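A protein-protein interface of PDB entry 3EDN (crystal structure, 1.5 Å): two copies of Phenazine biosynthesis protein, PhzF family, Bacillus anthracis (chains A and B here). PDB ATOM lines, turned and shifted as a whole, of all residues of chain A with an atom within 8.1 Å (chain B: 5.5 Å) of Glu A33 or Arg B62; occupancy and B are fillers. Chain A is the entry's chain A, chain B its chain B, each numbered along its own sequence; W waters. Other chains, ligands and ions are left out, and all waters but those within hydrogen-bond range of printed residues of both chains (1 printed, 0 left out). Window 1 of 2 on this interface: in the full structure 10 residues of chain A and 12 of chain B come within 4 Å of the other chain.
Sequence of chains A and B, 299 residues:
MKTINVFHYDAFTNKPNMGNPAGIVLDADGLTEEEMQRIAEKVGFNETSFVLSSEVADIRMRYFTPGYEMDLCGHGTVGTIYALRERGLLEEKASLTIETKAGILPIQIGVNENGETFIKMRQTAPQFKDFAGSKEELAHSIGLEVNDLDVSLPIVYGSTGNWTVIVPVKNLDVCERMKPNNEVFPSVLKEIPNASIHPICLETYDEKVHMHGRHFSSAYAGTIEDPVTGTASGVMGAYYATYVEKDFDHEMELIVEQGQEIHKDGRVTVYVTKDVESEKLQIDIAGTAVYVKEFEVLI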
ATOM      1  N   ALA A  28      -3.799 -20.422   1.606  1.00  0.00           N
ATOM      2  CA  ALA A  28      -3.261 -21.335   2.609  1.00  0.00           C
ATOM      3  C   ALA A  28      -1.897 -21.901   2.222  1.00  0.00           C
ATOM      4  O   ALA A  28      -1.442 -22.871   2.824  1.00  0.00           O
ATOM      5  CB  ALA A  28      -4.270 -22.488   2.848  1.00  0.00           C
ATOM      6  N   GLY A  30       0.936 -20.989   2.840  1.00  0.00           N
ATOM      7  CA  GLY A  30       1.929 -20.899   3.921  1.00  0.00           C
ATOM      8  C   GLY A  30       1.760 -21.863   5.084  1.00  0.00           C
ATOM      9  O   GLY A  30       2.454 -21.731   6.098  1.00  0.00           O
ATOM     10  N   LEU A  31       0.859 -22.837   4.936  1.00  0.00           N
ATOM     11  CA  LEU A  31       0.447 -23.700   6.053  1.00  0.00           C
ATOM     12  C   LEU A  31       0.710 -25.178   5.795  1.00  0.00           C
ATOM     13  O   LEU A  31       0.570 -25.662   4.680  1.00  0.00           O
ATOM     14  CB  LEU A  31      -1.057 -23.545   6.298  1.00  0.00           C
ATOM     15  CG  LEU A  31      -1.475 -22.131   6.692  1.00  0.00           C
ATOM     16  CD1 LEU A  31      -2.968 -21.977   6.631  1.00  0.00           C
ATOM     17  CD2 LEU A  31      -0.946 -21.819   8.090  1.00  0.00           C
ATOM     18  N   THR A  32       1.075 -25.904   6.848  1.00  0.00           N
ATOM     19  CA  THR A  32       1.120 -27.356   6.784  1.00  0.00           C
ATOM     20  C   THR A  32      -0.267 -27.943   7.042  1.00  0.00           C
ATOM     21  O   THR A  32      -1.156 -27.262   7.568  1.00  0.00           O
ATOM     22  CB  THR A  32       2.036 -27.937   7.858  1.00  0.00           C
ATOM     23  OG1 THR A  32       1.460 -27.697   9.157  1.00  0.00           O
ATOM     24  CG2 THR A  32       3.428 -27.277   7.789  1.00  0.00           C
ATOM     25  N   GLU A  33      -0.432 -29.211   6.691  1.00  0.00           N
ATOM     26  CA  GLU A  33      -1.670 -29.927   6.974  1.00  0.00           C
ATOM     27  C   GLU A  33      -1.981 -29.982   8.475  1.00  0.00           C
ATOM     28  O   GLU A  33      -3.148 -29.989   8.868  1.00  0.00           O
ATOM     29  CB  GLU A  33      -1.638 -31.326   6.347  1.00  0.00           C
ATOM     30  CG  GLU A  33      -0.658 -32.305   6.953  1.00  0.00           C
ATOM     31  CD  GLU A  33       0.810 -31.987   6.673  1.00  0.00           C
ATOM     32  OE1 GLU A  33       1.109 -31.301   5.676  1.00  0.00           O
ATOM     33  OE2 GLU A  33       1.666 -32.439   7.464  1.00  0.00           O
ATOM     34  N   GLU A  34      -0.957 -30.010   9.323  1.00  0.00           N
ATOM     35  CA  GLU A  34      -1.209 -30.033  10.757  1.00  0.00           C
ATOM     36  C   GLU A  34      -1.738 -28.689  11.223  1.00  0.00           C
ATOM     37  O   GLU A  34      -2.650 -28.621  12.061  1.00  0.00           O
ATOM     38  CB  GLU A  34       0.057 -30.409  11.515  1.00  0.00           C
ATOM     39  CG  GLU A  34       0.418 -31.869  11.307  1.00  0.00           C
ATOM     40  CD  GLU A  34       1.542 -32.324  12.224  1.00  0.00           C
ATOM     41  OE1 GLU A  34       1.576 -31.877  13.389  1.00  0.00           O
ATOM     42  OE2 GLU A  34       2.370 -33.150  11.773  1.00  0.00           O
ATOM     43  N   GLU A  35      -1.170 -27.620  10.677  1.00  0.00           N
ATOM     44  CA  GLU A  35      -1.668 -26.287  10.946  1.00  0.00           C
ATOM     45  C   GLU A  35      -3.100 -26.120  10.453  1.00  0.00           C
ATOM     46  O   GLU A  35      -3.922 -25.516  11.137  1.00  0.00           O
ATOM     47  CB  GLU A  35      -0.755 -25.247  10.312  1.00  0.00           C
ATOM     48  CG  GLU A  35       0.578 -25.144  11.039  1.00  0.00           C
ATOM     49  CD  GLU A  35       1.551 -24.205  10.362  1.00  0.00           C
ATOM     50  OE1 GLU A  35       1.608 -24.176   9.110  1.00  0.00           O
ATOM     51  OE2 GLU A  35       2.280 -23.507  11.099  1.00  0.00           O
ATOM     52  N   MET A  36      -3.396 -26.624   9.260  1.00  0.00           N
ATOM     53  CA  MET A  36      -4.757 -26.514   8.757  1.00  0.00           C
ATOM     54  C   MET A  36      -5.763 -27.190   9.692  1.00  0.00           C
ATOM     55  O   MET A  36      -6.817 -26.637  10.005  1.00  0.00           O
ATOM     56  CB  MET A  36      -4.868 -27.100   7.362  1.00  0.00           C
ATOM     57  CG  MET A  36      -4.039 -26.356   6.356  1.00  0.00           C
ATOM     58  SD  MET A  36      -4.233 -27.108   4.570  1.00  0.00           S
ATOM     59  CE  MET A  36      -2.466 -26.736   3.874  1.00  0.00           C
ATOM     60  N   GLN A  37      -5.419 -28.386  10.160  1.00  0.00           N
ATOM     61  CA  GLN A  37      -6.298 -29.117  11.062  1.00  0.00           C
ATOM     62  C   GLN A  37      -6.502 -28.342  12.382  1.00  0.00           C
ATOM     63  O   GLN A  37      -7.629 -28.234  12.902  1.00  0.00           O
ATOM     64  CB  GLN A  37      -5.735 -30.509  11.318  1.00  0.00           C
ATOM     65  CG  GLN A  37      -6.592 -31.317  12.258  1.00  0.00           C
ATOM     66  CD  GLN A  37      -7.931 -31.662  11.646  1.00  0.00           C
ATOM     67  OE1 GLN A  37      -8.036 -32.593  10.826  1.00  0.00           O
ATOM     68  NE2 GLN A  37      -8.970 -30.906  12.024  1.00  0.00           N
ATOM     69  N   ARG A  38      -5.420 -27.762  12.899  1.00  0.00           N
ATOM     70  CA  ARG A  38      -5.496 -26.977  14.127  1.00  0.00           C
ATOM     71  C   ARG A  38      -6.318 -25.708  13.939  1.00  0.00           C
ATOM     72  O   ARG A  38      -7.073 -25.311  14.827  1.00  0.00           O
ATOM     73  CB  ARG A  38      -4.097 -26.645  14.649  1.00  0.00           C
ATOM     74  CG  ARG A  38      -3.387 -27.878  15.179  1.00  0.00           C
ATOM     75  CD  ARG A  38      -1.919 -27.596  15.492  1.00  0.00           C
ATOM     76  NE  ARG A  38      -1.745 -26.502  16.443  1.00  0.00           N
ATOM     77  CZ  ARG A  38      -0.981 -25.435  16.219  1.00  0.00           C
ATOM     78  NH1 ARG A  38      -0.297 -25.337  15.075  1.00  0.00           N
ATOM     79  NH2 ARG A  38      -0.887 -24.478  17.146  1.00  0.00           N
ATOM     80  N   ILE A  39      -6.151 -25.056  12.794  1.00  0.00           N
ATOM     81  CA  ILE A  39      -6.949 -23.871  12.512  1.00  0.00           C
ATOM     82  C   ILE A  39      -8.428 -24.244  12.464  1.00  0.00           C
ATOM     83  O   ILE A  39      -9.266 -23.564  13.053  1.00  0.00           O
ATOM     84  CB  ILE A  39      -6.526 -23.219  11.187  1.00  0.00           C
ATOM     85  CG1 ILE A  39      -5.175 -22.513  11.330  1.00  0.00           C
ATOM     86  CG2 ILE A  39      -7.586 -22.221  10.713  1.00  0.00           C
ATOM     87  CD1 ILE A  39      -4.446 -22.272  10.004  1.00  0.00           C
ATOM     88  N   ALA A  40      -8.752 -25.333  11.785  1.00  0.00           N
ATOM     89  CA  ALA A  40     -10.149 -25.746  11.707  1.00  0.00           C
ATOM     90  C   ALA A  40     -10.712 -26.056  13.099  1.00  0.00           C
ATOM     91  O   ALA A  40     -11.876 -25.774  13.373  1.00  0.00           O
ATOM     92  CB  ALA A  40     -10.322 -26.938  10.769  1.00  0.00           C
ATOM     93  N   PHE A  50      -9.402 -24.425   2.761  1.00  0.00           N
ATOM     94  CA  PHE A  50      -8.090 -23.840   2.570  1.00  0.00           C
ATOM     95  C   PHE A  50      -7.773 -23.798   1.084  1.00  0.00           C
ATOM     96  O   PHE A  50      -7.801 -24.833   0.416  1.00  0.00           O
ATOM     97  CB  PHE A  50      -7.079 -24.706   3.308  1.00  0.00           C
ATOM     98  CG  PHE A  50      -7.314 -24.727   4.790  1.00  0.00           C
ATOM     99  CD1 PHE A  50      -6.655 -23.819   5.607  1.00  0.00           C
ATOM    100  CD2 PHE A  50      -8.210 -25.616   5.359  1.00  0.00           C
ATOM    101  CE1 PHE A  50      -6.877 -23.797   6.971  1.00  0.00           C
ATOM    102  CE2 PHE A  50      -8.452 -25.593   6.729  1.00  0.00           C
ATOM    103  CZ  PHE A  50      -7.779 -24.692   7.533  1.00  0.00           C
ATOM    104  N   LEU A  52      -5.424 -23.357  -2.106  1.00  0.00           N
ATOM    105  CA  LEU A  52      -4.032 -23.777  -2.330  1.00  0.00           C
ATOM    106  C   LEU A  52      -3.664 -23.742  -3.810  1.00  0.00           C
ATOM    107  O   LEU A  52      -4.534 -23.667  -4.683  1.00  0.00           O
ATOM    108  CB  LEU A  52      -3.847 -25.205  -1.814  1.00  0.00           C
ATOM    109  CG  LEU A  52      -4.111 -25.324  -0.312  1.00  0.00           C
ATOM    110  CD1 LEU A  52      -4.494 -26.726   0.133  1.00  0.00           C
ATOM    111  CD2 LEU A  52      -2.865 -24.881   0.425  1.00  0.00           C
ATOM    112  N   ARG A  62      -8.447 -27.845   0.213  1.00  0.00           N
ATOM    113  CA  ARG A  62      -8.576 -28.889   1.225  1.00  0.00           C
ATOM    114  C   ARG A  62      -9.668 -28.473   2.199  1.00  0.00           C
ATOM    115  O   ARG A  62      -9.865 -27.269   2.453  1.00  0.00           O
ATOM    116  CB  ARG A  62      -7.237 -29.158   1.923  1.00  0.00           C
ATOM    117  CG  ARG A  62      -6.211 -29.807   0.985  1.00  0.00           C
ATOM    118  CD  ARG A  62      -4.843 -29.991   1.646  1.00  0.00           C
ATOM    119  NE  ARG A  62      -4.805 -31.136   2.534  1.00  0.00           N
ATOM    120  CZ  ARG A  62      -3.693 -31.681   3.019  1.00  0.00           C
ATOM    121  NH1 ARG A  62      -2.488 -31.182   2.696  1.00  0.00           N
ATOM    122  NH2 ARG A  62      -3.787 -32.744   3.808  1.00  0.00           N
ATOM    123  N   PHE A  64     -11.554 -29.217   6.020  1.00  0.00           N
ATOM    124  CA  PHE A  64     -11.375 -29.823   7.342  1.00  0.00           C
ATOM    125  C   PHE A  64     -12.543 -29.536   8.264  1.00  0.00           C
ATOM    126  O   PHE A  64     -13.026 -28.411   8.317  1.00  0.00           O
ATOM    127  CB  PHE A  64     -10.125 -29.262   8.032  1.00  0.00           C
ATOM    128  CG  PHE A  64      -8.836 -29.714   7.437  1.00  0.00           C
ATOM    129  CD1 PHE A  64      -8.123 -30.755   8.022  1.00  0.00           C
ATOM    130  CD2 PHE A  64      -8.318 -29.088   6.306  1.00  0.00           C
ATOM    131  CE1 PHE A  64      -6.913 -31.186   7.491  1.00  0.00           C
ATOM    132  CE2 PHE A  64      -7.114 -29.503   5.777  1.00  0.00           C
ATOM    133  CZ  PHE A  64      -6.409 -30.560   6.370  1.00  0.00           C
ATOM    134  N   GLU A  69      -9.900 -34.363   8.139  1.00  0.00           N
ATOM    135  CA  GLU A  69      -9.949 -33.863   6.762  1.00  0.00           C
ATOM    136  C   GLU A  69     -11.013 -34.589   5.955  1.00  0.00           C
ATOM    137  O   GLU A  69     -11.136 -35.818   6.026  1.00  0.00           O
ATOM    138  CB  GLU A  69      -8.585 -34.014   6.070  1.00  0.00           C
ATOM    139  CG  GLU A  69      -8.542 -33.292   4.722  1.00  0.00           C
ATOM    140  CD  GLU A  69      -7.184 -33.331   4.047  1.00  0.00           C
ATOM    141  OE1 GLU A  69      -6.241 -33.956   4.592  1.00  0.00           O
ATOM    142  OE2 GLU A  69      -7.072 -32.712   2.972  1.00  0.00           O
ATOM    143  N   LYS A 101      -9.030 -34.135  -3.243  1.00  0.00           N
ATOM    144  CA  LYS A 101      -8.629 -35.512  -3.023  1.00  0.00           C
ATOM    145  C   LYS A 101      -9.611 -36.489  -3.671  1.00  0.00           C
ATOM    146  O   LYS A 101      -9.266 -37.648  -3.913  1.00  0.00           O
ATOM    147  CB  LYS A 101      -8.438 -35.786  -1.526  1.00  0.00           C
ATOM    148  CG  LYS A 101      -7.188 -35.104  -0.966  1.00  0.00           C
ATOM    149  CD  LYS A 101      -6.875 -35.523   0.461  1.00  0.00           C
ATOM    150  CE  LYS A 101      -5.548 -34.939   0.908  1.00  0.00           C
ATOM    151  NZ  LYS A 101      -5.239 -35.401   2.286  1.00  0.00           N
ATOM    152  N   GLU B  33       1.882 -33.315   1.740  1.00  0.00           N
ATOM    153  CA  GLU B  33       2.930 -34.048   2.470  1.00  0.00           C
ATOM    154  C   GLU B  33       3.124 -35.443   1.896  1.00  0.00           C
ATOM    155  O   GLU B  33       4.262 -35.898   1.738  1.00  0.00           O
ATOM    156  CB  GLU B  33       2.623 -34.166   3.969  1.00  0.00           C
ATOM    157  CG  GLU B  33       3.739 -34.832   4.799  1.00  0.00           C
ATOM    158  CD  GLU B  33       3.761 -36.363   4.723  1.00  0.00           C
ATOM    159  OE1 GLU B  33       2.813 -36.962   4.174  1.00  0.00           O
ATOM    160  OE2 GLU B  33       4.735 -36.970   5.227  1.00  0.00           O
ATOM    161  N   MET B  36       5.059 -35.129  -1.329  1.00  0.00           N
ATOM    162  CA  MET B  36       6.460 -34.792  -1.037  1.00  0.00           C
ATOM    163  C   MET B  36       7.217 -36.029  -0.545  1.00  0.00           C
ATOM    164  O   MET B  36       8.335 -36.309  -0.989  1.00  0.00           O
ATOM    165  CB  MET B  36       6.561 -33.650  -0.030  1.00  0.00           C
ATOM    166  CG  MET B  36       5.897 -32.369  -0.494  1.00  0.00           C
ATOM    167  SD  MET B  36       6.233 -30.880   0.716  1.00  0.00           S
ATOM    168  CE  MET B  36       4.407 -30.256   0.969  1.00  0.00           C
ATOM    169  N   GLU B  47      18.284 -37.018   1.705  1.00  0.00           N
ATOM    170  CA  GLU B  47      17.267 -36.004   1.973  1.00  0.00           C
ATOM    171  C   GLU B  47      16.905 -35.246   0.703  1.00  0.00           C
ATOM    172  O   GLU B  47      17.787 -34.951  -0.109  1.00  0.00           O
ATOM    173  CB  GLU B  47      17.781 -35.033   3.041  1.00  0.00           C
ATOM    174  CG  GLU B  47      16.763 -34.034   3.528  1.00  0.00           C
ATOM    175  CD  GLU B  47      16.770 -32.736   2.741  1.00  0.00           C
ATOM    176  OE1 GLU B  47      17.767 -32.474   2.039  1.00  0.00           O
ATOM    177  OE2 GLU B  47      15.773 -31.972   2.833  1.00  0.00           O
ATOM    178  N   THR B  48      15.606 -34.972   0.537  1.00  0.00           N
ATOM    179  CA  THR B  48      15.048 -34.095  -0.505  1.00  0.00           C
ATOM    180  C   THR B  48      14.264 -32.980   0.174  1.00  0.00           C
ATOM    181  O   THR B  48      13.484 -33.246   1.102  1.00  0.00           O
ATOM    182  CB  THR B  48      14.143 -34.864  -1.483  1.00  0.00           C
ATOM    183  OG1 THR B  48      14.952 -35.819  -2.191  1.00  0.00           O
ATOM    184  CG2 THR B  48      13.483 -33.916  -2.495  1.00  0.00           C
ATOM    185  N   SER B  49      14.497 -31.743  -0.277  1.00  0.00           N
ATOM    186  CA  SER B  49      13.923 -30.543   0.344  1.00  0.00           C
ATOM    187  C   SER B  49      12.870 -29.961  -0.562  1.00  0.00           C
ATOM    188  O   SER B  49      12.987 -30.054  -1.787  1.00  0.00           O
ATOM    189  CB  SER B  49      15.002 -29.466   0.586  1.00  0.00           C
ATOM    190  OG  SER B  49      16.021 -29.888   1.491  1.00  0.00           O
ATOM    191  N   PHE B  50      11.882 -29.287   0.035  1.00  0.00           N
ATOM    192  CA  PHE B  50      10.751 -28.748  -0.709  1.00  0.00           C
ATOM    193  C   PHE B  50      10.589 -27.282  -0.352  1.00  0.00           C
ATOM    194  O   PHE B  50      10.460 -26.958   0.821  1.00  0.00           O
ATOM    195  CB  PHE B  50       9.505 -29.563  -0.354  1.00  0.00           C
ATOM    196  CG  PHE B  50       9.598 -30.993  -0.840  1.00  0.00           C
ATOM    197  CD1 PHE B  50       9.071 -31.380  -2.084  1.00  0.00           C
ATOM    198  CD2 PHE B  50      10.271 -31.934  -0.070  1.00  0.00           C
ATOM    199  CE1 PHE B  50       9.202 -32.704  -2.532  1.00  0.00           C
ATOM    200  CE2 PHE B  50      10.406 -33.260  -0.515  1.00  0.00           C
ATOM    201  CZ  PHE B  50       9.883 -33.629  -1.746  1.00  0.00           C
ATOM    202  N   VAL B  51      10.602 -26.405  -1.365  1.00  0.00           N
ATOM    203  CA  VAL B  51      10.494 -24.971  -1.146  1.00  0.00           C
ATOM    204  C   VAL B  51       9.035 -24.544  -1.226  1.00  0.00           C
ATOM    205  O   VAL B  51       8.359 -24.824  -2.210  1.00  0.00           O
ATOM    206  CB  VAL B  51      11.348 -24.213  -2.187  1.00  0.00           C
ATOM    207  CG1 VAL B  51      11.204 -22.693  -2.047  1.00  0.00           C
ATOM    208  CG2 VAL B  51      12.798 -24.631  -2.073  1.00  0.00           C
ATOM    209  N   LEU B  52       8.583 -23.858  -0.178  1.00  0.00           N
ATOM    210  CA  LEU B  52       7.167 -23.556   0.035  1.00  0.00           C
ATOM    211  C   LEU B  52       6.973 -22.085   0.400  1.00  0.00           C
ATOM    212  O   LEU B  52       7.924 -21.401   0.811  1.00  0.00           O
ATOM    213  CB  LEU B  52       6.624 -24.445   1.157  1.00  0.00           C
ATOM    214  CG  LEU B  52       6.690 -25.952   0.878  1.00  0.00           C
ATOM    215  CD1 LEU B  52       6.924 -26.745   2.144  1.00  0.00           C
ATOM    216  CD2 LEU B  52       5.452 -26.420   0.116  1.00  0.00           C
ATOM    217  N   ARG B  60       9.682 -21.023   3.079  1.00  0.00           N
ATOM    218  CA  ARG B  60       9.464 -22.101   4.018  1.00  0.00           C
ATOM    219  C   ARG B  60      10.067 -23.371   3.422  1.00  0.00           C
ATOM    220  O   ARG B  60      10.116 -23.528   2.198  1.00  0.00           O
ATOM    221  CB  ARG B  60       7.962 -22.250   4.269  1.00  0.00           C
ATOM    222  CG  ARG B  60       7.581 -23.373   5.232  1.00  0.00           C
ATOM    223  CD  ARG B  60       6.131 -23.211   5.692  1.00  0.00           C
ATOM    224  NE  ARG B  60       5.169 -23.330   4.585  1.00  0.00           N
ATOM    225  CZ  ARG B  60       4.544 -24.455   4.242  1.00  0.00           C
ATOM    226  NH1 ARG B  60       4.780 -25.580   4.904  1.00  0.00           N
ATOM    227  NH2 ARG B  60       3.687 -24.460   3.228  1.00  0.00           N
ATOM    228  N   MET B  61      10.547 -24.271   4.271  1.00  0.00           N
ATOM    229  CA  MET B  61      11.108 -25.511   3.737  1.00  0.00           C
ATOM    230  C   MET B  61      10.637 -26.686   4.548  1.00  0.00           C
ATOM    231  O   MET B  61      10.515 -26.578   5.764  1.00  0.00           O
ATOM    232  CB  MET B  61      12.632 -25.500   3.803  1.00  0.00           C
ATOM    233  CG  MET B  61      13.278 -24.628   2.772  1.00  0.00           C
ATOM    234  SD  MET B  61      15.208 -24.827   2.785  1.00  0.00           S
ATOM    235  CE  MET B  61      15.373 -26.558   2.166  1.00  0.00           C
ATOM    236  N   ARG B  62      10.399 -27.795   3.853  1.00  0.00           N
ATOM    237  CA  ARG B  62      10.202 -29.092   4.495  1.00  0.00           C
ATOM    238  C   ARG B  62      11.244 -30.072   3.979  1.00  0.00           C
ATOM    239  O   ARG B  62      11.678 -29.983   2.832  1.00  0.00           O
ATOM    240  CB  ARG B  62       8.774 -29.608   4.283  1.00  0.00           C
ATOM    241  CG  ARG B  62       7.779 -28.800   5.111  1.00  0.00           C
ATOM    242  CD  ARG B  62       6.338 -29.253   4.907  1.00  0.00           C
ATOM    243  NE  ARG B  62       6.036 -30.486   5.635  1.00  0.00           N
ATOM    244  CZ  ARG B  62       4.801 -30.986   5.751  1.00  0.00           C
ATOM    245  NH1 ARG B  62       3.759 -30.360   5.196  1.00  0.00           N
ATOM    246  NH2 ARG B  62       4.616 -32.105   6.437  1.00  0.00           N
ATOM    247  N   TYR B  63      11.660 -30.988   4.852  1.00  0.00           N
ATOM    248  CA  TYR B  63      12.793 -31.878   4.575  1.00  0.00           C
ATOM    249  C   TYR B  63      12.340 -33.322   4.712  1.00  0.00           C
ATOM    250  O   TYR B  63      11.710 -33.654   5.700  1.00  0.00           O
ATOM    251  CB  TYR B  63      13.879 -31.648   5.602  1.00  0.00           C
ATOM    252  CG  TYR B  63      14.316 -30.216   5.798  1.00  0.00           C
ATOM    253  CD1 TYR B  63      15.181 -29.595   4.899  1.00  0.00           C
ATOM    254  CD2 TYR B  63      13.915 -29.504   6.914  1.00  0.00           C
ATOM    255  CE1 TYR B  63      15.608 -28.302   5.104  1.00  0.00           C
ATOM    256  CE2 TYR B  63      14.327 -28.210   7.127  1.00  0.00           C
ATOM    257  CZ  TYR B  63      15.185 -27.600   6.214  1.00  0.00           C
ATOM    258  OH  TYR B  63      15.624 -26.301   6.426  1.00  0.00           O
ATOM    259  N   PHE B  64      12.654 -34.175   3.737  1.00  0.00           N
ATOM    260  CA  PHE B  64      12.239 -35.580   3.820  1.00  0.00           C
ATOM    261  C   PHE B  64      13.371 -36.545   3.484  1.00  0.00           C
ATOM    262  O   PHE B  64      14.111 -36.329   2.528  1.00  0.00           O
ATOM    263  CB  PHE B  64      11.094 -35.866   2.856  1.00  0.00           C
ATOM    264  CG  PHE B  64       9.805 -35.186   3.212  1.00  0.00           C
ATOM    265  CD1 PHE B  64       8.795 -35.875   3.883  1.00  0.00           C
ATOM    266  CD2 PHE B  64       9.597 -33.862   2.854  1.00  0.00           C
ATOM    267  CE1 PHE B  64       7.600 -35.248   4.207  1.00  0.00           C
ATOM    268  CE2 PHE B  64       8.410 -33.227   3.170  1.00  0.00           C
ATOM    269  CZ  PHE B  64       7.406 -33.917   3.840  1.00  0.00           C
ATOM    270  N   GLU B  69       9.710 -37.618   7.381  1.00  0.00           N
ATOM    271  CA  GLU B  69      10.041 -36.205   7.415  1.00  0.00           C
ATOM    272  C   GLU B  69      11.039 -35.889   8.528  1.00  0.00           C
ATOM    273  O   GLU B  69      10.995 -36.483   9.615  1.00  0.00           O
ATOM    274  CB  GLU B  69       8.760 -35.390   7.590  1.00  0.00           C
ATOM    275  CG  GLU B  69       8.997 -33.902   7.484  1.00  0.00           C
ATOM    276  CD  GLU B  69       7.721 -33.079   7.447  1.00  0.00           C
ATOM    277  OE1 GLU B  69       6.606 -33.637   7.578  1.00  0.00           O
ATOM    278  OE2 GLU B  69       7.848 -31.857   7.301  1.00  0.00           O
ATOM    279  N   MET B  70      11.947 -34.952   8.261  1.00  0.00           N
ATOM    280  CA  MET B  70      12.850 -34.455   9.283  1.00  0.00           C
ATOM    281  C   MET B  70      12.583 -33.004   9.646  1.00  0.00           C
ATOM    282  O   MET B  70      12.038 -32.242   8.847  1.00  0.00           O
ATOM    283  CB  MET B  70      14.309 -34.635   8.852  1.00  0.00           C
ATOM    284  CG  MET B  70      14.804 -36.072   9.014  1.00  0.00           C
ATOM    285  SD  MET B  70      16.716 -36.153   8.684  1.00  0.00           S
ATOM    286  CE  MET B  70      16.694 -35.177   7.015  1.00  0.00           C
ATOM    287  N   LYS B 101       9.424 -26.282  10.435  1.00  0.00           N
ATOM    288  CA  LYS B 101       8.601 -26.778  11.525  1.00  0.00           C
ATOM    289  C   LYS B 101       9.265 -26.548  12.880  1.00  0.00           C
ATOM    290  O   LYS B 101       8.584 -26.317  13.880  1.00  0.00           O
ATOM    291  CB  LYS B 101       8.308 -28.260  11.321  1.00  0.00           C
ATOM    292  CG  LYS B 101       7.239 -28.513  10.278  1.00  0.00           C
ATOM    293  CD  LYS B 101       7.185 -29.987   9.944  1.00  0.00           C
ATOM    294  CE  LYS B 101       5.826 -30.412   9.513  1.00  0.00           C
ATOM    295  NZ  LYS B 101       5.713 -31.877   9.715  1.00  0.00           N
HETATM  296  O   HOH W   1       2.860 -31.072   9.300  1.00  0.00           O
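Water W1 lies within hydrogen-bond range of the side-chain carboxylate (OE2) of Glu A33 (2.6 Å), the side-chain amino group (NZ) of Lys B101 (3.0 Å) and the side-chain carboxylate (OE2) of Glu A34 (3.3 Å).
Of the printed residues of chain B, Gly A30 touches Arg B60.
Of the printed residues of chain B, Leu A31 touches Arg B60 (3.6 Å).
Printed residues of chain B within 4 Å of Thr A32: Arg B60 (3.6 Å) and Arg B62 (3.99 Å).
Of the printed residues of chain B, Glu A33 touches Glu B33 and Arg B62.
Thr B48 touches none of the printed residues of chain A.
Of the printed residues of chain A, Arg B60 touches Gly A30, Leu A31 and Thr A32.
Of the printed residues of chain A, Arg B62 touches Thr A32 (3.99 Å) and Glu A33 (2.9 Å).
Tyr B63 touches none of the printed residues of chain A.
The nearest printed residue of chain B that does not touch Glu A33 is Lys B101 (4.7 Å).
NH2 of Arg B60 touches O of Leu A31, 3.6 Å away.
CG2 of Thr A32 touches NH1 of Arg B60, 3.6 Å away.
Arg B62 touches Thr A32 (NH1 to CB, 3.99 Å).
Glu A33 touches Glu B33.
The side-chain carboxylate (OE1) of Glu A33 lies within salt-bridge range of the guanidinium group (NH1) of Arg B62, at 2.9 Å.
The backbone carbonyl oxygen (O) of Gly A30 sits at hydrogen-bond distance from the guanidinium group (NE) of Arg B60, 3.5 Å away.
Glu A33 touches its own counterpart, Glu B33.
Glu A33 touches Arg B62, but with the chains exchanged Arg A62 does not touch Glu B33 (5.0 Å).
Of the 6 pairs that touch across the chains among the printed residues, 1 has its exchanged pair printed and touching as well.
Of the 18 printed residues of chain A, 4 touch a printed residue of chain B.
Of the 16 printed residues of chain B, 3 touch a printed residue of chain A.
Along chain B the printed residues that touch a printed residue of chain A span positions 33 to 62.
Among the printed residues, 6 pairs touch across the chains.
Among the printed residues, Asp or Glu carboxylates within 4 Å of a Lys or Arg side-chain nitrogen of the other chain: Glu A33 with Arg B62 (2.9 Å).
N of Thr A32 sits at hydrogen-bond distance from OE1 of Glu A35 (2.9 Å).
The backbone NH of Phe B50 is in hydrogen-bond range of the backbone carbonyl oxygen of Arg B62 (2.9 Å).
OE1 of Glu B69 is in salt-bridge range of NH2 of Arg B62 (2.8 Å).
The backbone NH of Leu B52 sits at hydrogen-bond distance from the backbone carbonyl oxygen of Arg B60, at 2.8 Å.
The side-chain hydroxyl (OG1) of Thr A32 lies close to the backbone NH (N) of Glu A34 (3.3 Å).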
